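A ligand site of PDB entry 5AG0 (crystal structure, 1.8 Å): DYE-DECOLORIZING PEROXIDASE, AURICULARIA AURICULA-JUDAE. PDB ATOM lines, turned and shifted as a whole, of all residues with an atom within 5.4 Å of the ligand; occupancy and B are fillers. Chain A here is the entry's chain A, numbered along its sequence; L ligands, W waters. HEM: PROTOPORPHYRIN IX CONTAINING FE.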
ATOM      1  N   GLU A 160      20.445 -15.032  -3.281  1.00  0.00           N
ATOM      2  CA  GLU A 160      21.385 -15.953  -3.920  1.00  0.00           C
ATOM      3  C   GLU A 160      22.735 -15.888  -3.205  1.00  0.00           C
ATOM      4  O   GLU A 160      22.891 -15.152  -2.225  1.00  0.00           O
ATOM      5  CB  GLU A 160      21.513 -15.672  -5.415  1.00  0.00           C
ATOM      6  CG  GLU A 160      21.778 -14.210  -5.774  1.00  0.00           C
ATOM      7  CD  GLU A 160      23.180 -13.782  -5.397  1.00  0.00           C
ATOM      8  OE1 GLU A 160      24.154 -14.479  -5.788  1.00  0.00           O
ATOM      9  OE2 GLU A 160      23.316 -12.780  -4.665  1.00  0.00           O
ATOM     10  N   PHE A 162      25.726 -14.729  -3.621  1.00  0.00           N
ATOM     11  CA  PHE A 162      26.501 -13.502  -3.468  1.00  0.00           C
ATOM     12  C   PHE A 162      25.874 -12.611  -2.393  1.00  0.00           C
ATOM     13  O   PHE A 162      26.482 -11.648  -1.929  1.00  0.00           O
ATOM     14  CB  PHE A 162      26.601 -12.727  -4.787  1.00  0.00           C
ATOM     15  CG  PHE A 162      27.512 -13.363  -5.804  1.00  0.00           C
ATOM     16  CD1 PHE A 162      28.688 -13.977  -5.424  1.00  0.00           C
ATOM     17  CD2 PHE A 162      27.200 -13.299  -7.157  1.00  0.00           C
ATOM     18  CE1 PHE A 162      29.522 -14.556  -6.371  1.00  0.00           C
ATOM     19  CE2 PHE A 162      28.038 -13.869  -8.105  1.00  0.00           C
ATOM     20  CZ  PHE A 162      29.199 -14.498  -7.712  1.00  0.00           C
ATOM     21  N   PHE A 164      22.485 -11.375  -2.597  1.00  0.00           N
ATOM     22  CA  PHE A 164      21.505 -10.438  -3.151  1.00  0.00           C
ATOM     23  C   PHE A 164      20.101 -11.045  -3.217  1.00  0.00           C
ATOM     24  O   PHE A 164      19.926 -12.170  -3.683  1.00  0.00           O
ATOM     25  CB  PHE A 164      21.932  -9.959  -4.540  1.00  0.00           C
ATOM     26  CG  PHE A 164      23.154  -9.089  -4.523  1.00  0.00           C
ATOM     27  CD1 PHE A 164      24.417  -9.642  -4.435  1.00  0.00           C
ATOM     28  CD2 PHE A 164      23.039  -7.710  -4.606  1.00  0.00           C
ATOM     29  CE1 PHE A 164      25.549  -8.842  -4.396  1.00  0.00           C
ATOM     30  CE2 PHE A 164      24.164  -6.897  -4.577  1.00  0.00           C
ATOM     31  CZ  PHE A 164      25.413  -7.466  -4.466  1.00  0.00           C
ATOM     32  N   LEU A 165      19.108 -10.283  -2.753  1.00  0.00           N
ATOM     33  CA  LEU A 165      17.728 -10.721  -2.921  1.00  0.00           C
ATOM     34  C   LEU A 165      17.454 -11.043  -4.380  1.00  0.00           C
ATOM     35  O   LEU A 165      17.761 -10.257  -5.270  1.00  0.00           O
ATOM     36  CB  LEU A 165      16.741  -9.658  -2.427  1.00  0.00           C
ATOM     37  CG  LEU A 165      15.280 -10.106  -2.334  1.00  0.00           C
ATOM     38  CD1 LEU A 165      15.123 -11.226  -1.321  1.00  0.00           C
ATOM     39  CD2 LEU A 165      14.372  -8.941  -1.979  1.00  0.00           C
ATOM     40  N   ASP A 166      16.928 -12.244  -4.613  1.00  0.00           N
ATOM     41  CA  ASP A 166      16.604 -12.671  -5.955  1.00  0.00           C
ATOM     42  C   ASP A 166      15.095 -12.904  -6.077  1.00  0.00           C
ATOM     43  O   ASP A 166      14.376 -12.917  -5.074  1.00  0.00           O
ATOM     44  CB  ASP A 166      17.369 -13.950  -6.303  1.00  0.00           C
ATOM     45  CG  ASP A 166      17.500 -14.145  -7.799  1.00  0.00           C
ATOM     46  OD1 ASP A 166      16.658 -13.616  -8.543  1.00  0.00           O
ATOM     47  OD2 ASP A 166      18.468 -14.819  -8.220  1.00  0.00           O
ATOM     48  N   GLY A 167      14.617 -13.048  -7.299  1.00  0.00           N
ATOM     49  CA  GLY A 167      13.210 -13.370  -7.535  1.00  0.00           C
ATOM     50  C   GLY A 167      12.256 -12.193  -7.336  1.00  0.00           C
ATOM     51  O   GLY A 167      11.058 -12.396  -7.133  1.00  0.00           O
ATOM     52  N   ILE A 168      12.775 -10.983  -7.445  1.00  0.00           N
ATOM     53  CA  ILE A 168      11.926  -9.795  -7.490  1.00  0.00           C
ATOM     54  C   ILE A 168      11.238  -9.667  -8.847  1.00  0.00           C
ATOM     55  O   ILE A 168      10.029  -9.491  -8.934  1.00  0.00           O
ATOM     56  CB  ILE A 168      12.734  -8.521  -7.220  1.00  0.00           C
ATOM     57  CG1 ILE A 168      13.320  -8.541  -5.810  1.00  0.00           C
ATOM     58  CG2 ILE A 168      11.881  -7.286  -7.457  1.00  0.00           C
ATOM     59  CD1 ILE A 168      14.606  -7.766  -5.670  1.00  0.00           C
ATOM     60  N   ALA A 169      12.029  -9.751  -9.920  1.00  0.00           N
ATOM     61  CA  ALA A 169      11.564  -9.354 -11.232  1.00  0.00           C
ATOM     62  C   ALA A 169      11.181 -10.555 -12.087  1.00  0.00           C
ATOM     63  O   ALA A 169      11.954 -11.495 -12.243  1.00  0.00           O
ATOM     64  CB  ALA A 169      12.621  -8.515 -11.940  1.00  0.00           C
ATOM     65  N   GLN A 170       9.963 -10.534 -12.625  1.00  0.00           N
ATOM     66  CA  GLN A 170       9.500 -11.524 -13.590  1.00  0.00           C
ATOM     67  C   GLN A 170       8.594 -10.808 -14.587  1.00  0.00           C
ATOM     68  O   GLN A 170       7.966  -9.809 -14.237  1.00  0.00           O
ATOM     69  CB  GLN A 170       8.698 -12.617 -12.893  1.00  0.00           C
ATOM     70  CG  GLN A 170       9.387 -13.281 -11.709  1.00  0.00           C
ATOM     71  CD  GLN A 170      10.364 -14.358 -12.142  1.00  0.00           C
ATOM     72  OE1 GLN A 170      10.694 -14.478 -13.320  1.00  0.00           O
ATOM     73  NE2 GLN A 170      10.846 -15.143 -11.185  1.00  0.00           N
ATOM     74  N   LEU A 217      25.463 -23.033 -12.388  1.00  0.00           N
ATOM     75  CA  LEU A 217      26.365 -21.906 -12.382  1.00  0.00           C
ATOM     76  C   LEU A 217      27.056 -21.755 -11.034  1.00  0.00           C
ATOM     77  O   LEU A 217      26.450 -21.318 -10.053  1.00  0.00           O
ATOM     78  CB  LEU A 217      25.615 -20.620 -12.741  1.00  0.00           C
ATOM     79  CG  LEU A 217      24.884 -20.680 -14.094  1.00  0.00           C
ATOM     80  CD1 LEU A 217      24.195 -19.363 -14.410  1.00  0.00           C
ATOM     81  CD2 LEU A 217      25.851 -21.072 -15.198  1.00  0.00           C
ATOM     82  N   GLN A 219      29.270 -20.185  -8.212  1.00  0.00           N
ATOM     83  CA  GLN A 219      29.617 -18.819  -7.847  1.00  0.00           C
ATOM     84  C   GLN A 219      30.809 -18.811  -6.902  1.00  0.00           C
ATOM     85  O   GLN A 219      30.847 -19.548  -5.922  1.00  0.00           O
ATOM     86  CB  GLN A 219      28.419 -18.140  -7.187  1.00  0.00           C
ATOM     87  CG  GLN A 219      27.241 -17.949  -8.143  1.00  0.00           C
ATOM     88  CD  GLN A 219      26.003 -17.467  -7.429  1.00  0.00           C
ATOM     89  OE1 GLN A 219      25.015 -18.199  -7.313  1.00  0.00           O
ATOM     90  NE2 GLN A 219      26.039 -16.241  -6.926  1.00  0.00           N
ATOM     91  N   VAL A 251      25.417  -5.631  -9.930  1.00  0.00           N
ATOM     92  CA  VAL A 251      24.158  -6.361 -10.003  1.00  0.00           C
ATOM     93  C   VAL A 251      23.058  -5.473 -10.573  1.00  0.00           C
ATOM     94  O   VAL A 251      22.247  -5.919 -11.394  1.00  0.00           O
ATOM     95  CB  VAL A 251      23.734  -6.884  -8.614  1.00  0.00           C
ATOM     96  CG1 VAL A 251      22.345  -7.507  -8.681  1.00  0.00           C
ATOM     97  CG2 VAL A 251      24.745  -7.899  -8.084  1.00  0.00           C
ATOM     98  N   ARG A 253      21.185  -3.986  -8.239  1.00  0.00           N
ATOM     99  CA  ARG A 253      20.389  -3.905  -7.015  1.00  0.00           C
ATOM    100  C   ARG A 253      21.309  -4.034  -5.807  1.00  0.00           C
ATOM    101  O   ARG A 253      22.371  -4.656  -5.896  1.00  0.00           O
ATOM    102  CB  ARG A 253      19.345  -5.027  -6.964  1.00  0.00           C
ATOM    103  CG  ARG A 253      18.227  -4.907  -7.988  1.00  0.00           C
ATOM    104  CD  ARG A 253      17.176  -5.987  -7.775  1.00  0.00           C
ATOM    105  NE  ARG A 253      16.110  -5.885  -8.765  1.00  0.00           N
ATOM    106  CZ  ARG A 253      15.093  -5.035  -8.701  1.00  0.00           C
ATOM    107  NH1 ARG A 253      14.937  -4.268  -7.622  1.00  0.00           N
ATOM    108  NH2 ARG A 253      14.197  -5.001  -9.671  1.00  0.00           N
ATOM    109  N   ASN A 279      10.497  -2.426  -8.222  1.00  0.00           N
ATOM    110  CA  ASN A 279      10.668  -2.622  -9.653  1.00  0.00           C
ATOM    111  C   ASN A 279      10.139  -1.457 -10.472  1.00  0.00           C
ATOM    112  O   ASN A 279      10.061  -1.523 -11.702  1.00  0.00           O
ATOM    113  CB  ASN A 279      10.011  -3.922 -10.112  1.00  0.00           C
ATOM    114  CG  ASN A 279      10.783  -4.603 -11.224  1.00  0.00           C
ATOM    115  OD1 ASN A 279      11.990  -4.391 -11.378  1.00  0.00           O
ATOM    116  ND2 ASN A 279      10.097  -5.420 -12.011  1.00  0.00           N
ATOM    117  N   TYR A 283      14.919   3.294 -15.814  1.00  0.00           N
ATOM    118  CA  TYR A 283      16.293   3.759 -16.058  1.00  0.00           C
ATOM    119  C   TYR A 283      16.385   5.222 -16.507  1.00  0.00           C
ATOM    120  O   TYR A 283      17.463   5.816 -16.494  1.00  0.00           O
ATOM    121  CB  TYR A 283      17.056   2.851 -17.029  1.00  0.00           C
ATOM    122  CG  TYR A 283      17.358   1.485 -16.435  1.00  0.00           C
ATOM    123  CD1 TYR A 283      17.947   1.360 -15.186  1.00  0.00           C
ATOM    124  CD2 TYR A 283      17.011   0.322 -17.112  1.00  0.00           C
ATOM    125  CE1 TYR A 283      18.179   0.129 -14.624  1.00  0.00           C
ATOM    126  CE2 TYR A 283      17.248  -0.923 -16.560  1.00  0.00           C
ATOM    127  CZ  TYR A 283      17.839  -1.016 -15.312  1.00  0.00           C
ATOM    128  OH  TYR A 283      18.079  -2.251 -14.760  1.00  0.00           O
ATOM    129  N   HIS A 302      24.033  -6.101 -14.227  1.00  0.00           N
ATOM    130  CA  HIS A 302      23.378  -7.365 -14.606  1.00  0.00           C
ATOM    131  C   HIS A 302      21.917  -7.209 -15.004  1.00  0.00           C
ATOM    132  O   HIS A 302      21.509  -7.686 -16.065  1.00  0.00           O
ATOM    133  CB  HIS A 302      23.530  -8.399 -13.489  1.00  0.00           C
ATOM    134  CG  HIS A 302      22.787  -9.677 -13.747  1.00  0.00           C
ATOM    135  ND1 HIS A 302      23.032 -10.491 -14.826  1.00  0.00           N
ATOM    136  CD2 HIS A 302      21.864 -10.331 -12.994  1.00  0.00           C
ATOM    137  CE1 HIS A 302      22.269 -11.563 -14.768  1.00  0.00           C
ATOM    138  NE2 HIS A 302      21.535 -11.480 -13.673  1.00  0.00           N
ATOM    139  N   ILE A 303      21.103  -6.609 -14.140  1.00  0.00           N
ATOM    140  CA  ILE A 303      19.674  -6.505 -14.451  1.00  0.00           C
ATOM    141  C   ILE A 303      19.380  -5.590 -15.642  1.00  0.00           C
ATOM    142  O   ILE A 303      18.398  -5.790 -16.351  1.00  0.00           O
ATOM    143  CB  ILE A 303      18.807  -6.116 -13.238  1.00  0.00           C
ATOM    144  CG1 ILE A 303      19.155  -4.712 -12.722  1.00  0.00           C
ATOM    145  CG2 ILE A 303      18.949  -7.146 -12.120  1.00  0.00           C
ATOM    146  CD1 ILE A 303      18.062  -4.098 -11.874  1.00  0.00           C
ATOM    147  N   THR A 306      20.025  -7.615 -18.787  1.00  0.00           N
ATOM    148  CA  THR A 306      19.079  -8.703 -19.020  1.00  0.00           C
ATOM    149  C   THR A 306      17.633  -8.230 -19.188  1.00  0.00           C
ATOM    150  O   THR A 306      16.818  -8.934 -19.797  1.00  0.00           O
ATOM    151  CB  THR A 306      19.151  -9.792 -17.924  1.00  0.00           C
ATOM    152  OG1 THR A 306      19.042  -9.185 -16.640  1.00  0.00           O
ATOM    153  CG2 THR A 306      20.477 -10.541 -18.015  1.00  0.00           C
ATOM    154  N   ARG A 307      17.309  -7.074 -18.641  1.00  0.00           N
ATOM    155  CA  ARG A 307      16.101  -6.341 -19.048  1.00  0.00           C
ATOM    156  C   ARG A 307      16.412  -4.856 -19.202  1.00  0.00           C
ATOM    157  O   ARG A 307      16.431  -4.108 -18.225  1.00  0.00           O
ATOM    158  CB  ARG A 307      14.948  -6.537 -18.055  1.00  0.00           C
ATOM    159  CG  ARG A 307      13.630  -5.947 -18.539  1.00  0.00           C
ATOM    160  CD  ARG A 307      12.628  -5.702 -17.421  1.00  0.00           C
ATOM    161  NE  ARG A 307      11.509  -4.889 -17.899  1.00  0.00           N
ATOM    162  CZ  ARG A 307      10.609  -4.290 -17.114  1.00  0.00           C
ATOM    163  NH1 ARG A 307      10.648  -4.452 -15.800  1.00  0.00           N
ATOM    164  NH2 ARG A 307       9.650  -3.544 -17.662  1.00  0.00           N
ATOM    165  N   ARG A 309      14.920  -2.300 -20.425  1.00  0.00           N
ATOM    166  CA  ARG A 309      13.869  -1.302 -20.245  1.00  0.00           C
ATOM    167  C   ARG A 309      14.008  -0.151 -21.235  1.00  0.00           C
ATOM    168  O   ARG A 309      14.066  -0.369 -22.451  1.00  0.00           O
ATOM    169  CB  ARG A 309      13.824  -0.831 -18.788  1.00  0.00           C
ATOM    170  CG  ARG A 309      13.723  -1.996 -17.793  1.00  0.00           C
ATOM    171  CD  ARG A 309      13.495  -1.571 -16.344  1.00  0.00           C
ATOM    172  NE  ARG A 309      13.701  -2.723 -15.456  1.00  0.00           N
ATOM    173  CZ  ARG A 309      13.032  -2.945 -14.329  1.00  0.00           C
ATOM    174  NH1 ARG A 309      12.132  -2.081 -13.886  1.00  0.00           N
ATOM    175  NH2 ARG A 309      13.260  -4.061 -13.645  1.00  0.00           N
ATOM    176  N   ILE A 328      12.208 -13.850 -19.764  1.00  0.00           N
ATOM    177  CA  ILE A 328      12.234 -15.205 -19.237  1.00  0.00           C
ATOM    178  C   ILE A 328      11.576 -15.258 -17.859  1.00  0.00           C
ATOM    179  O   ILE A 328      11.606 -14.278 -17.115  1.00  0.00           O
ATOM    180  CB  ILE A 328      13.671 -15.763 -19.129  1.00  0.00           C
ATOM    181  CG1 ILE A 328      14.555 -14.850 -18.286  1.00  0.00           C
ATOM    182  CG2 ILE A 328      14.271 -15.957 -20.521  1.00  0.00           C
ATOM    183  CD1 ILE A 328      15.892 -15.464 -17.924  1.00  0.00           C
ATOM    184  N   ARG A 330      12.065 -16.911 -14.308  1.00  0.00           N
ATOM    185  CA  ARG A 330      13.201 -17.483 -13.590  1.00  0.00           C
ATOM    186  C   ARG A 330      12.748 -18.294 -12.390  1.00  0.00           C
ATOM    187  O   ARG A 330      11.981 -17.811 -11.551  1.00  0.00           O
ATOM    188  CB  ARG A 330      14.183 -16.391 -13.170  1.00  0.00           C
ATOM    189  CG  ARG A 330      14.930 -15.750 -14.335  1.00  0.00           C
ATOM    190  CD  ARG A 330      15.796 -14.577 -13.881  1.00  0.00           C
ATOM    191  NE  ARG A 330      15.003 -13.592 -13.139  1.00  0.00           N
ATOM    192  CZ  ARG A 330      15.287 -13.176 -11.912  1.00  0.00           C
ATOM    193  NH1 ARG A 330      16.381 -13.607 -11.299  1.00  0.00           N
ATOM    194  NH2 ARG A 330      14.475 -12.339 -11.288  1.00  0.00           N
ATOM    195  N   LEU A 355      24.270 -21.187  -8.241  1.00  0.00           N
ATOM    196  CA  LEU A 355      22.858 -21.081  -8.605  1.00  0.00           C
ATOM    197  C   LEU A 355      22.491 -22.216  -9.541  1.00  0.00           C
ATOM    198  O   LEU A 355      23.118 -22.394 -10.584  1.00  0.00           O
ATOM    199  CB  LEU A 355      22.602 -19.738  -9.285  1.00  0.00           C
ATOM    200  CG  LEU A 355      21.146 -19.398  -9.623  1.00  0.00           C
ATOM    201  CD1 LEU A 355      20.330 -19.275  -8.346  1.00  0.00           C
ATOM    202  CD2 LEU A 355      21.074 -18.124 -10.436  1.00  0.00           C
ATOM    203  N   PHE A 357      20.364 -22.589 -12.057  1.00  0.00           N
ATOM    204  CA  PHE A 357      19.650 -21.596 -12.845  1.00  0.00           C
ATOM    205  C   PHE A 357      18.605 -22.285 -13.709  1.00  0.00           C
ATOM    206  O   PHE A 357      18.894 -23.271 -14.391  1.00  0.00           O
ATOM    207  CB  PHE A 357      20.629 -20.797 -13.705  1.00  0.00           C
ATOM    208  CG  PHE A 357      19.966 -19.842 -14.660  1.00  0.00           C
ATOM    209  CD1 PHE A 357      19.643 -18.554 -14.274  1.00  0.00           C
ATOM    210  CD2 PHE A 357      19.692 -20.233 -15.968  1.00  0.00           C
ATOM    211  CE1 PHE A 357      19.036 -17.672 -15.156  1.00  0.00           C
ATOM    212  CE2 PHE A 357      19.090 -19.364 -16.850  1.00  0.00           C
ATOM    213  CZ  PHE A 357      18.757 -18.082 -16.443  1.00  0.00           C
ATOM    214  N   PHE A 368      16.783 -17.200 -22.780  1.00  0.00           N
ATOM    215  CA  PHE A 368      18.060 -17.356 -22.108  1.00  0.00           C
ATOM    216  C   PHE A 368      19.232 -17.199 -23.084  1.00  0.00           C
ATOM    217  O   PHE A 368      20.176 -16.444 -22.832  1.00  0.00           O
ATOM    218  CB  PHE A 368      18.152 -18.708 -21.408  1.00  0.00           C
ATOM    219  CG  PHE A 368      19.563 -19.176 -21.196  1.00  0.00           C
ATOM    220  CD1 PHE A 368      20.356 -18.576 -20.232  1.00  0.00           C
ATOM    221  CD2 PHE A 368      20.120 -20.125 -22.031  1.00  0.00           C
ATOM    222  CE1 PHE A 368      21.677 -18.956 -20.069  1.00  0.00           C
ATOM    223  CE2 PHE A 368      21.451 -20.499 -21.890  1.00  0.00           C
ATOM    224  CZ  PHE A 368      22.230 -19.914 -20.904  1.00  0.00           C
ATOM    225  N   LEU A 371      19.622 -13.492 -24.176  1.00  0.00           N
ATOM    226  CA  LEU A 371      20.146 -12.683 -23.088  1.00  0.00           C
ATOM    227  C   LEU A 371      21.642 -12.914 -22.876  1.00  0.00           C
ATOM    228  O   LEU A 371      22.404 -11.961 -22.722  1.00  0.00           O
ATOM    229  CB  LEU A 371      19.366 -12.960 -21.797  1.00  0.00           C
ATOM    230  CG  LEU A 371      18.136 -12.081 -21.536  1.00  0.00           C
ATOM    231  CD1 LEU A 371      17.291 -11.940 -22.794  1.00  0.00           C
ATOM    232  CD2 LEU A 371      17.297 -12.666 -20.410  1.00  0.00           C
ATOM    233  N   GLN A 372      22.065 -14.172 -22.890  1.00  0.00           N
ATOM    234  CA  GLN A 372      23.461 -14.502 -22.625  1.00  0.00           C
ATOM    235  C   GLN A 372      24.378 -14.045 -23.751  1.00  0.00           C
ATOM    236  O   GLN A 372      25.386 -13.369 -23.507  1.00  0.00           O
ATOM    237  CB  GLN A 372      23.621 -16.009 -22.367  1.00  0.00           C
ATOM    238  CG  GLN A 372      25.043 -16.432 -22.036  1.00  0.00           C
ATOM    239  CD  GLN A 372      25.466 -15.989 -20.645  1.00  0.00           C
ATOM    240  OE1 GLN A 372      24.847 -16.344 -19.645  1.00  0.00           O
ATOM    241  NE2 GLN A 372      26.545 -15.220 -20.580  1.00  0.00           N
ATOM    242  N   ILE A 395      28.338 -10.099 -13.910  1.00  0.00           N
ATOM    243  CA  ILE A 395      27.898 -11.315 -13.217  1.00  0.00           C
ATOM    244  C   ILE A 395      27.976 -12.540 -14.126  1.00  0.00           C
ATOM    245  O   ILE A 395      28.544 -13.558 -13.744  1.00  0.00           O
ATOM    246  CB  ILE A 395      26.481 -11.155 -12.633  1.00  0.00           C
ATOM    247  CG1 ILE A 395      26.411  -9.902 -11.745  1.00  0.00           C
ATOM    248  CG2 ILE A 395      26.086 -12.395 -11.845  1.00  0.00           C
ATOM    249  CD1 ILE A 395      27.363  -9.917 -10.560  1.00  0.00           C
ATOM    250  N   ILE A 396      27.392 -12.446 -15.315  1.00  0.00           N
ATOM    251  CA  ILE A 396      27.293 -13.610 -16.193  1.00  0.00           C
ATOM    252  C   ILE A 396      28.023 -13.475 -17.519  1.00  0.00           C
ATOM    253  O   ILE A 396      28.095 -14.433 -18.296  1.00  0.00           O
ATOM    254  CB  ILE A 396      25.817 -13.982 -16.470  1.00  0.00           C
ATOM    255  CG1 ILE A 396      25.103 -12.823 -17.187  1.00  0.00           C
ATOM    256  CG2 ILE A 396      25.102 -14.317 -15.167  1.00  0.00           C
ATOM    257  CD1 ILE A 396      23.795 -13.235 -17.827  1.00  0.00           C
ATOM    258  N   VAL A 424      31.346 -16.240 -11.863  1.00  0.00           N
ATOM    259  CA  VAL A 424      30.413 -17.313 -12.127  1.00  0.00           C
ATOM    260  C   VAL A 424      31.038 -18.254 -13.142  1.00  0.00           C
ATOM    261  O   VAL A 424      31.518 -17.825 -14.195  1.00  0.00           O
ATOM    262  CB  VAL A 424      29.095 -16.771 -12.723  1.00  0.00           C
ATOM    263  CG1 VAL A 424      28.154 -17.919 -13.067  1.00  0.00           C
ATOM    264  CG2 VAL A 424      28.424 -15.824 -11.743  1.00  0.00           C
HETATM  265  CHA HEM L   1      17.942 -10.662 -12.011  1.00  0.00           C
HETATM  266  CHB HEM L   1      21.752 -12.799  -9.896  1.00  0.00           C
HETATM  267  CHC HEM L   1      22.371 -15.583 -13.857  1.00  0.00           C
HETATM  268  CHD HEM L   1      18.799 -13.179 -16.070  1.00  0.00           C
HETATM  269  C1A HEM L   1      18.914 -11.021 -11.121  1.00  0.00           C
HETATM  270  C2A HEM L   1      19.042 -10.475  -9.826  1.00  0.00           C
HETATM  271  C3A HEM L   1      20.115 -11.060  -9.231  1.00  0.00           C
HETATM  272  C4A HEM L   1      20.644 -12.002 -10.144  1.00  0.00           C
HETATM  273  CMA HEM L   1      20.636 -10.807  -7.832  1.00  0.00           C
HETATM  274  CAA HEM L   1      18.165  -9.388  -9.224  1.00  0.00           C
HETATM  275  CBA HEM L   1      16.916  -9.982  -8.592  1.00  0.00           C
HETATM  276  CGA HEM L   1      15.680  -9.632  -9.390  1.00  0.00           C
HETATM  277  O1A HEM L   1      15.584  -8.555 -10.019  1.00  0.00           O
HETATM  278  O2A HEM L   1      14.723 -10.436  -9.409  1.00  0.00           O
HETATM  279  C1B HEM L   1      22.243 -13.757 -10.794  1.00  0.00           C
HETATM  280  C2B HEM L   1      23.323 -14.638 -10.503  1.00  0.00           C
HETATM  281  C3B HEM L   1      23.507 -15.439 -11.595  1.00  0.00           C
HETATM  282  C4B HEM L   1      22.485 -15.011 -12.589  1.00  0.00           C
HETATM  283  CMB HEM L   1      24.112 -14.680  -9.218  1.00  0.00           C
HETATM  284  CAB HEM L   1      24.508 -16.495 -11.809  1.00  0.00           C
HETATM  285  CBB HEM L   1      24.834 -17.347 -10.844  1.00  0.00           C
HETATM  286  C1C HEM L   1      21.466 -15.146 -14.814  1.00  0.00           C
HETATM  287  C2C HEM L   1      21.455 -15.578 -16.154  1.00  0.00           C
HETATM  288  C3C HEM L   1      20.430 -14.886 -16.795  1.00  0.00           C
HETATM  289  C4C HEM L   1      19.841 -14.026 -15.835  1.00  0.00           C
HETATM  290  CMC HEM L   1      22.354 -16.642 -16.739  1.00  0.00           C
HETATM  291  CAC HEM L   1      19.981 -15.039 -18.202  1.00  0.00           C
HETATM  292  CBC HEM L   1      20.864 -15.188 -19.194  1.00  0.00           C
HETATM  293  C1D HEM L   1      18.302 -12.343 -15.071  1.00  0.00           C
HETATM  294  C2D HEM L   1      17.110 -11.535 -15.338  1.00  0.00           C
HETATM  295  C3D HEM L   1      16.868 -10.828 -14.229  1.00  0.00           C
HETATM  296  C4D HEM L   1      17.907 -11.232 -13.267  1.00  0.00           C
HETATM  297  CMD HEM L   1      16.337 -11.500 -16.636  1.00  0.00           C
HETATM  298  CAD HEM L   1      15.745  -9.832 -14.011  1.00  0.00           C
HETATM  299  CBD HEM L   1      15.995  -8.545 -14.812  1.00  0.00           C
HETATM  300  CGD HEM L   1      14.805  -7.605 -14.778  1.00  0.00           C
HETATM  301  O1D HEM L   1      13.659  -8.013 -15.085  1.00  0.00           O
HETATM  302  O2D HEM L   1      14.959  -6.403 -14.470  1.00  0.00           O
HETATM  303  NA  HEM L   1      19.924 -11.928 -11.316  1.00  0.00           N
HETATM  304  NB  HEM L   1      21.799 -14.002 -12.031  1.00  0.00           N
HETATM  305  NC  HEM L   1      20.547 -14.159 -14.671  1.00  0.00           N
HETATM  306  ND  HEM L   1      18.769 -12.129 -13.817  1.00  0.00           N
HETATM  307 FE   HEM L   1      20.209 -13.010 -12.965  1.00  0.00          FE
HETATM  308  O   HOH W   1      11.354  -6.684 -14.351  1.00  0.00           O
HETATM  309  O   HOH W   2      12.537 -10.360 -15.884  1.00  0.00           O
HETATM  310  O   HOH W   3      15.332  -6.462 -11.735  1.00  0.00           O
HETATM  311  O   HOH W   4      16.198  -4.093 -15.628  1.00  0.00           O
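N of Gly 167 is in hydrogen-bond range of O2A of the ligand, 3.4 Å away.
The backbone NH (N) of Ala 169 sits at hydrogen-bond distance from an oxygen (O2A) of the ligand (2.8 Å).
NH2 of Arg 330 is in salt-bridge range of O2A of the ligand.
A ring nitrogen (NE2) of His 302 binds an iron atom (FE) of the ligand (2.1 Å).
O1A of the ligand lies within salt-bridge range of NE of Arg 253, at 3.0 Å.
The guanidinium group of Arg 309 lies within salt-bridge range of an oxygen (O2D) of the ligand (3.0 Å).
N of Ile 168 sits at hydrogen-bond distance from O2A of the ligand, 2.8 Å away.
O of His 302 is in hydrogen-bond range of OG1 of Thr 306 (2.9 Å).
The backbone NH (N) of Phe 162 lies within hydrogen-bond range of the side-chain carboxylate (OE1) of Glu 160 (2.7 Å).
The side-chain amide nitrogen (NE2) of Gln 219 is in hydrogen-bond range of the side-chain carboxylate (OE1) of Glu 160 (2.8 Å).
O of Val 251 is in hydrogen-bond range of N of Ile 303 (3.1 Å).
OE1 of Gln 219 is in hydrogen-bond range of N of Leu 355 (3.2 Å).
The side-chain amide oxygen of Asn 279 sits at hydrogen-bond distance from the guanidinium group of Arg 309, at 2.6 Å.
NH1 of Arg 330 is in salt-bridge range of OD1 of Asp 166, 2.8 Å away.
The guanidinium group (NH2) of Arg 330 lies within hydrogen-bond range of the backbone carbonyl oxygen (O) of Ala 169, at 2.8 Å.
Merely in contact with the ligand: Glu 160 (3.4 Å), Phe 162 (3.96 Å), Phe 164 (3.6 Å), Leu 165 (3.4 Å), Asp 166 (3.6 Å), Leu 217 (3.9 Å), Gln 219 (3.4 Å), Val 251 (3.8 Å), Ile 303 (3.7 Å), Thr 306 (3.3 Å), Arg 307 (3.4 Å), Leu 355 (3.6 Å), Phe 357 (3.4 Å), Phe 368 (3.6 Å), Leu 371 (3.7 Å), Gln 372 (3.8 Å), Ile 395 (3.8 Å), Ile 396 (3.3 Å) and Val 424 (3.97 Å).
26 residues have an atom within 4 Å of the ligand: Glu 160, Phe 162, Phe 164, Leu 165, Asp 166, Gly 167, Ile 168, Ala 169, Leu 217, Gln 219, Val 251, Arg 253, His 302, Ile 303, Thr 306, Arg 307, Arg 309, Arg 330, Leu 355, Phe 357, Phe 368, Leu 371, Gln 372, Ile 395, Ile 396 and Val 424.
The nearest printed residue that does not touch the ligand is Ile 328 (4.1 Å).
Water W3 bridges O1A of the ligand (2.7 Å) and NH2 of Arg 253 (2.8 Å).
Water W4 lies within hydrogen-bond range of O of Arg 307 (2.6 Å), OH of Tyr 283 (2.8 Å), NE of Arg 309 (2.9 Å), O2D of the ligand (2.9 Å) and O of Ile 303 (2.9 Å).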
